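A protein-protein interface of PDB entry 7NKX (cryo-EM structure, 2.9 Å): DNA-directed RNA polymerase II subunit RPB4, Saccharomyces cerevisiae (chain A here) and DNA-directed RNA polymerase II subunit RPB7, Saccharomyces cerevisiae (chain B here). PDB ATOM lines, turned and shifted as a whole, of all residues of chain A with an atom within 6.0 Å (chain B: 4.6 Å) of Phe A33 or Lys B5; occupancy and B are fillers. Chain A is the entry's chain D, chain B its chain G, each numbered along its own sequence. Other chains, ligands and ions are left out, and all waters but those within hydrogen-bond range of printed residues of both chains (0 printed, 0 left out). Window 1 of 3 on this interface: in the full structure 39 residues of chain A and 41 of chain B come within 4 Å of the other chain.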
ATOM      1  N   LEU A  29      16.731  -9.660  -3.294  1.00  0.00           N
ATOM      2  CA  LEU A  29      17.510  -8.939  -2.303  1.00  0.00           C
ATOM      3  C   LEU A  29      18.100  -7.656  -2.890  1.00  0.00           C
ATOM      4  O   LEU A  29      18.073  -7.415  -4.100  1.00  0.00           O
ATOM      5  CB  LEU A  29      18.626  -9.830  -1.758  1.00  0.00           C
ATOM      6  CG  LEU A  29      18.326 -10.824  -0.630  1.00  0.00           C
ATOM      7  CD1 LEU A  29      17.909 -10.114   0.652  1.00  0.00           C
ATOM      8  CD2 LEU A  29      17.272 -11.810  -1.042  1.00  0.00           C
ATOM      9  N   GLY A  30      18.641  -6.823  -1.998  1.00  0.00           N
ATOM     10  CA  GLY A  30      19.251  -5.572  -2.386  1.00  0.00           C
ATOM     11  C   GLY A  30      20.627  -5.755  -3.000  1.00  0.00           C
ATOM     12  O   GLY A  30      21.140  -6.863  -3.160  1.00  0.00           O
ATOM     13  N   GLN A  31      21.234  -4.619  -3.346  1.00  0.00           N
ATOM     14  CA  GLN A  31      22.506  -4.638  -4.067  1.00  0.00           C
ATOM     15  C   GLN A  31      23.649  -5.219  -3.230  1.00  0.00           C
ATOM     16  O   GLN A  31      24.607  -5.760  -3.793  1.00  0.00           O
ATOM     17  CB  GLN A  31      22.824  -3.221  -4.594  1.00  0.00           C
ATOM     18  CG  GLN A  31      22.787  -2.066  -3.574  1.00  0.00           C
ATOM     19  CD  GLN A  31      23.817  -2.196  -2.505  1.00  0.00           C
ATOM     20  OE1 GLN A  31      24.995  -2.400  -2.783  1.00  0.00           O
ATOM     21  NE2 GLN A  31      23.356  -2.275  -1.276  1.00  0.00           N
ATOM     22  N   GLU A  32      23.576  -5.121  -1.897  1.00  0.00           N
ATOM     23  CA  GLU A  32      24.605  -5.692  -1.031  1.00  0.00           C
ATOM     24  C   GLU A  32      24.346  -7.150  -0.713  1.00  0.00           C
ATOM     25  O   GLU A  32      25.284  -7.875  -0.364  1.00  0.00           O
ATOM     26  CB  GLU A  32      24.708  -4.973   0.327  1.00  0.00           C
ATOM     27  CG  GLU A  32      23.402  -4.807   1.123  1.00  0.00           C
ATOM     28  CD  GLU A  32      23.443  -3.638   2.081  1.00  0.00           C
ATOM     29  OE1 GLU A  32      23.097  -3.833   3.265  1.00  0.00           O
ATOM     30  OE2 GLU A  32      23.841  -2.535   1.669  1.00  0.00           O
ATOM     31  N   PHE A  33      23.096  -7.582  -0.825  1.00  0.00           N
ATOM     32  CA  PHE A  33      22.634  -8.838  -0.253  1.00  0.00           C
ATOM     33  C   PHE A  33      22.629  -9.940  -1.312  1.00  0.00           C
ATOM     34  O   PHE A  33      21.606 -10.550  -1.619  1.00  0.00           O
ATOM     35  CB  PHE A  33      21.250  -8.625   0.344  1.00  0.00           C
ATOM     36  CG  PHE A  33      21.245  -7.913   1.653  1.00  0.00           C
ATOM     37  CD1 PHE A  33      20.581  -6.705   1.791  1.00  0.00           C
ATOM     38  CD2 PHE A  33      21.814  -8.488   2.767  1.00  0.00           C
ATOM     39  CE1 PHE A  33      20.553  -6.056   3.004  1.00  0.00           C
ATOM     40  CE2 PHE A  33      21.779  -7.854   3.974  1.00  0.00           C
ATOM     41  CZ  PHE A  33      21.149  -6.634   4.101  1.00  0.00           C
ATOM     42  N   GLN A  34      23.810 -10.196  -1.864  1.00  0.00           N
ATOM     43  CA  GLN A  34      23.996 -11.340  -2.741  1.00  0.00           C
ATOM     44  C   GLN A  34      24.202 -12.602  -1.918  1.00  0.00           C
ATOM     45  O   GLN A  34      24.471 -12.562  -0.715  1.00  0.00           O
ATOM     46  CB  GLN A  34      25.191 -11.166  -3.693  1.00  0.00           C
ATOM     47  CG  GLN A  34      25.094 -10.099  -4.793  1.00  0.00           C
ATOM     48  CD  GLN A  34      24.755  -8.717  -4.313  1.00  0.00           C
ATOM     49  OE1 GLN A  34      25.240  -8.273  -3.275  1.00  0.00           O
ATOM     50  NE2 GLN A  34      23.919  -8.019  -5.075  1.00  0.00           N
ATOM     51  N   LEU A  35      24.058 -13.739  -2.594  1.00  0.00           N
ATOM     52  CA  LEU A  35      24.456 -15.007  -2.007  1.00  0.00           C
ATOM     53  C   LEU A  35      25.968 -15.117  -1.858  1.00  0.00           C
ATOM     54  O   LEU A  35      26.431 -15.940  -1.065  1.00  0.00           O
ATOM     55  CB  LEU A  35      23.890 -16.156  -2.858  1.00  0.00           C
ATOM     56  CG  LEU A  35      24.301 -17.615  -2.615  1.00  0.00           C
ATOM     57  CD1 LEU A  35      23.177 -18.532  -3.055  1.00  0.00           C
ATOM     58  CD2 LEU A  35      25.550 -18.000  -3.401  1.00  0.00           C
ATOM     59  N   GLN A  37      29.595 -13.229  -0.961  1.00  0.00           N
ATOM     60  CA  GLN A  37      30.239 -12.109  -0.285  1.00  0.00           C
ATOM     61  C   GLN A  37      31.760 -12.187  -0.412  1.00  0.00           C
ATOM     62  O   GLN A  37      32.362 -13.270  -0.461  1.00  0.00           O
ATOM     63  CB  GLN A  37      29.870 -12.049   1.214  1.00  0.00           C
ATOM     64  CG  GLN A  37      28.379 -11.943   1.595  1.00  0.00           C
ATOM     65  CD  GLN A  37      27.549 -11.085   0.652  1.00  0.00           C
ATOM     66  OE1 GLN A  37      26.993 -11.569  -0.328  1.00  0.00           O
ATOM     67  NE2 GLN A  37      27.467  -9.794   0.955  1.00  0.00           N
ATOM     68  N   LEU A  47      27.366 -16.207   1.617  1.00  0.00           N
ATOM     69  CA  LEU A  47      26.828 -15.519   2.780  1.00  0.00           C
ATOM     70  C   LEU A  47      26.559 -16.538   3.879  1.00  0.00           C
ATOM     71  O   LEU A  47      26.072 -17.641   3.613  1.00  0.00           O
ATOM     72  CB  LEU A  47      25.540 -14.781   2.401  1.00  0.00           C
ATOM     73  CG  LEU A  47      24.779 -13.941   3.437  1.00  0.00           C
ATOM     74  CD1 LEU A  47      25.692 -13.077   4.298  1.00  0.00           C
ATOM     75  CD2 LEU A  47      23.739 -13.071   2.740  1.00  0.00           C
ATOM     76  N   PHE B   3      22.837 -10.980  10.810  1.00  0.00           N
ATOM     77  CA  PHE B   3      23.791 -11.580   9.888  1.00  0.00           C
ATOM     78  C   PHE B   3      25.136 -10.967  10.221  1.00  0.00           C
ATOM     79  O   PHE B   3      25.189  -9.921  10.857  1.00  0.00           O
ATOM     80  CB  PHE B   3      23.483 -11.231   8.418  1.00  0.00           C
ATOM     81  CG  PHE B   3      22.513 -12.141   7.709  1.00  0.00           C
ATOM     82  CD1 PHE B   3      21.769 -13.106   8.361  1.00  0.00           C
ATOM     83  CD2 PHE B   3      22.352 -11.999   6.343  1.00  0.00           C
ATOM     84  CE1 PHE B   3      20.907 -13.909   7.670  1.00  0.00           C
ATOM     85  CE2 PHE B   3      21.487 -12.797   5.652  1.00  0.00           C
ATOM     86  CZ  PHE B   3      20.767 -13.751   6.316  1.00  0.00           C
ATOM     87  N   ILE B   4      26.209 -11.549   9.689  1.00  0.00           N
ATOM     88  CA  ILE B   4      27.561 -11.020   9.857  1.00  0.00           C
ATOM     89  C   ILE B   4      28.137 -10.577   8.519  1.00  0.00           C
ATOM     90  O   ILE B   4      28.245 -11.382   7.587  1.00  0.00           O
ATOM     91  CB  ILE B   4      28.476 -12.073  10.522  1.00  0.00           C
ATOM     92  CG1 ILE B   4      29.924 -11.569  10.668  1.00  0.00           C
ATOM     93  CG2 ILE B   4      28.464 -13.427   9.759  1.00  0.00           C
ATOM     94  CD1 ILE B   4      30.846 -12.548  11.375  1.00  0.00           C
ATOM     95  N   LYS B   5      28.484  -9.288   8.420  1.00  0.00           N
ATOM     96  CA  LYS B   5      29.046  -8.719   7.196  1.00  0.00           C
ATOM     97  C   LYS B   5      30.339  -7.970   7.485  1.00  0.00           C
ATOM     98  O   LYS B   5      30.498  -7.346   8.542  1.00  0.00           O
ATOM     99  CB  LYS B   5      28.104  -7.817   6.395  1.00  0.00           C
ATOM    100  CG  LYS B   5      27.442  -6.671   7.111  1.00  0.00           C
ATOM    101  CD  LYS B   5      26.051  -6.366   6.529  1.00  0.00           C
ATOM    102  CE  LYS B   5      25.026  -7.509   6.624  1.00  0.00           C
ATOM    103  NZ  LYS B   5      23.657  -7.042   6.312  1.00  0.00           N
ATOM    104  N   ASP B   6      31.281  -8.103   6.552  1.00  0.00           N
ATOM    105  CA  ASP B   6      32.576  -7.431   6.617  1.00  0.00           C
ATOM    106  C   ASP B   6      32.420  -6.015   6.079  1.00  0.00           C
ATOM    107  O   ASP B   6      31.962  -5.823   4.947  1.00  0.00           O
ATOM    108  CB  ASP B   6      33.664  -8.139   5.804  1.00  0.00           C
ATOM    109  CG  ASP B   6      33.189  -8.605   4.445  1.00  0.00           C
ATOM    110  OD1 ASP B   6      34.016  -9.153   3.694  1.00  0.00           O
ATOM    111  OD2 ASP B   6      31.989  -8.433   4.142  1.00  0.00           O
ATOM    112  N   LEU B   7      32.782  -5.033   6.896  1.00  0.00           N
ATOM    113  CA  LEU B   7      32.694  -3.621   6.571  1.00  0.00           C
ATOM    114  C   LEU B   7      34.031  -2.966   6.928  1.00  0.00           C
ATOM    115  O   LEU B   7      34.948  -3.614   7.456  1.00  0.00           O
ATOM    116  CB  LEU B   7      31.491  -2.979   7.277  1.00  0.00           C
ATOM    117  CG  LEU B   7      31.542  -2.766   8.790  1.00  0.00           C
ATOM    118  CD1 LEU B   7      32.278  -1.483   9.158  1.00  0.00           C
ATOM    119  CD2 LEU B   7      30.129  -2.773   9.376  1.00  0.00           C
ATOM    120  N   TYR B  74      36.613  -4.635   9.723  1.00  0.00           N
ATOM    121  CA  TYR B  74      36.040  -5.456  10.784  1.00  0.00           C
ATOM    122  C   TYR B  74      34.771  -6.110  10.267  1.00  0.00           C
ATOM    123  O   TYR B  74      34.286  -5.779   9.187  1.00  0.00           O
ATOM    124  CB  TYR B  74      35.796  -4.687  12.093  1.00  0.00           C
ATOM    125  CG  TYR B  74      34.688  -3.670  12.151  1.00  0.00           C
ATOM    126  CD1 TYR B  74      34.960  -2.317  12.023  1.00  0.00           C
ATOM    127  CD2 TYR B  74      33.381  -4.053  12.404  1.00  0.00           C
ATOM    128  CE1 TYR B  74      33.958  -1.383  12.107  1.00  0.00           C
ATOM    129  CE2 TYR B  74      32.374  -3.129  12.487  1.00  0.00           C
ATOM    130  CZ  TYR B  74      32.669  -1.795  12.349  1.00  0.00           C
ATOM    131  OH  TYR B  74      31.661  -0.866  12.426  1.00  0.00           O
ATOM    132  N   ARG B  75      34.270  -7.073  11.037  1.00  0.00           N
ATOM    133  CA  ARG B  75      33.032  -7.770  10.717  1.00  0.00           C
ATOM    134  C   ARG B  75      32.053  -7.402  11.817  1.00  0.00           C
ATOM    135  O   ARG B  75      32.464  -7.126  12.948  1.00  0.00           O
ATOM    136  CB  ARG B  75      33.216  -9.291  10.717  1.00  0.00           C
ATOM    137  CG  ARG B  75      34.251  -9.865   9.773  1.00  0.00           C
ATOM    138  CD  ARG B  75      33.590 -10.404   8.505  1.00  0.00           C
ATOM    139  NE  ARG B  75      32.964 -11.724   8.617  1.00  0.00           N
ATOM    140  CZ  ARG B  75      33.575 -12.865   8.940  1.00  0.00           C
ATOM    141  NH1 ARG B  75      34.873 -12.916   9.213  1.00  0.00           N
ATOM    142  NH2 ARG B  75      32.866 -13.984   8.997  1.00  0.00           N
ATOM    143  N   ALA B  76      30.759  -7.402  11.501  1.00  0.00           N
ATOM    144  CA  ALA B  76      29.789  -7.033  12.523  1.00  0.00           C
ATOM    145  C   ALA B  76      28.416  -7.617  12.240  1.00  0.00           C
ATOM    146  O   ALA B  76      28.072  -7.960  11.100  1.00  0.00           O
ATOM    147  CB  ALA B  76      29.686  -5.509  12.650  1.00  0.00           C
ATOM    148  N   VAL B  78      24.581  -6.973  12.036  1.00  0.00           N
ATOM    149  CA  VAL B  78      23.603  -5.924  11.764  1.00  0.00           C
ATOM    150  C   VAL B  78      22.196  -6.512  11.692  1.00  0.00           C
ATOM    151  O   VAL B  78      22.009  -7.698  11.406  1.00  0.00           O
ATOM    152  CB  VAL B  78      23.918  -5.127  10.484  1.00  0.00           C
ATOM    153  CG1 VAL B  78      25.091  -4.182  10.723  1.00  0.00           C
ATOM    154  CG2 VAL B  78      24.193  -6.030   9.340  1.00  0.00           C
ATOM    155  N   PHE B  82      12.758  -6.314   6.593  1.00  0.00           N
ATOM    156  CA  PHE B  82      12.313  -6.445   5.203  1.00  0.00           C
ATOM    157  C   PHE B  82      10.805  -6.676   5.149  1.00  0.00           C
ATOM    158  O   PHE B  82      10.206  -7.199   6.090  1.00  0.00           O
ATOM    159  CB  PHE B  82      12.992  -7.579   4.377  1.00  0.00           C
ATOM    160  CG  PHE B  82      14.316  -7.227   3.755  1.00  0.00           C
ATOM    161  CD1 PHE B  82      14.669  -7.836   2.561  1.00  0.00           C
ATOM    162  CD2 PHE B  82      15.205  -6.341   4.330  1.00  0.00           C
ATOM    163  CE1 PHE B  82      15.857  -7.557   1.939  1.00  0.00           C
ATOM    164  CE2 PHE B  82      16.411  -6.063   3.701  1.00  0.00           C
ATOM    165  CZ  PHE B  82      16.733  -6.675   2.509  1.00  0.00           C
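O of Leu A35 is in hydrogen-bond range of N of Leu A47, 2.9 Å away. The backbone carbonyl oxygen (O) of Phe B3 is in hydrogen-bond range of the backbone NH (N) of Val B78, 3.2 Å away. The backbone carbonyl oxygen of Lys B5 lies within hydrogen-bond range of the backbone NH of Ala B76 (3.0 Å).
Leu A29 touches Phe B82 (CD1 to CE1, 3.5 Å). Lys B5 touches Phe A33 (NZ to CE2, 3.1 Å). Phe A33 touches Phe B82 (CE1 to CZ, 3.9 Å). CD2 of Leu A47 touches CE2 of Phe B3, at 3.7 Å.
Printed residues of chain B within 4 Å of Leu A29: Phe B82. Phe A33 touches two residues of chain B. Of the printed residues of chain B, Leu A47 touches Phe B3. Of the printed residues of chain A, Phe B3 touches Leu A47. Lys B5 touches just one residue of chain A: Phe A33. Printed residues of chain A within 4 Å of Phe B82: Leu A29 and Phe A33. The nearest residue of chain A that does not touch Lys B5 is Glu A32 (4.5 Å).
Hydrophobic or aromatic side chains of chain A within 4 Å of the printed part of chain B: Leu A29, Phe A33 and Leu A47. Of the 10 printed residues of chain B, 3 touch a printed residue of chain A. Among the printed residues, 4 pairs touch across the chains.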
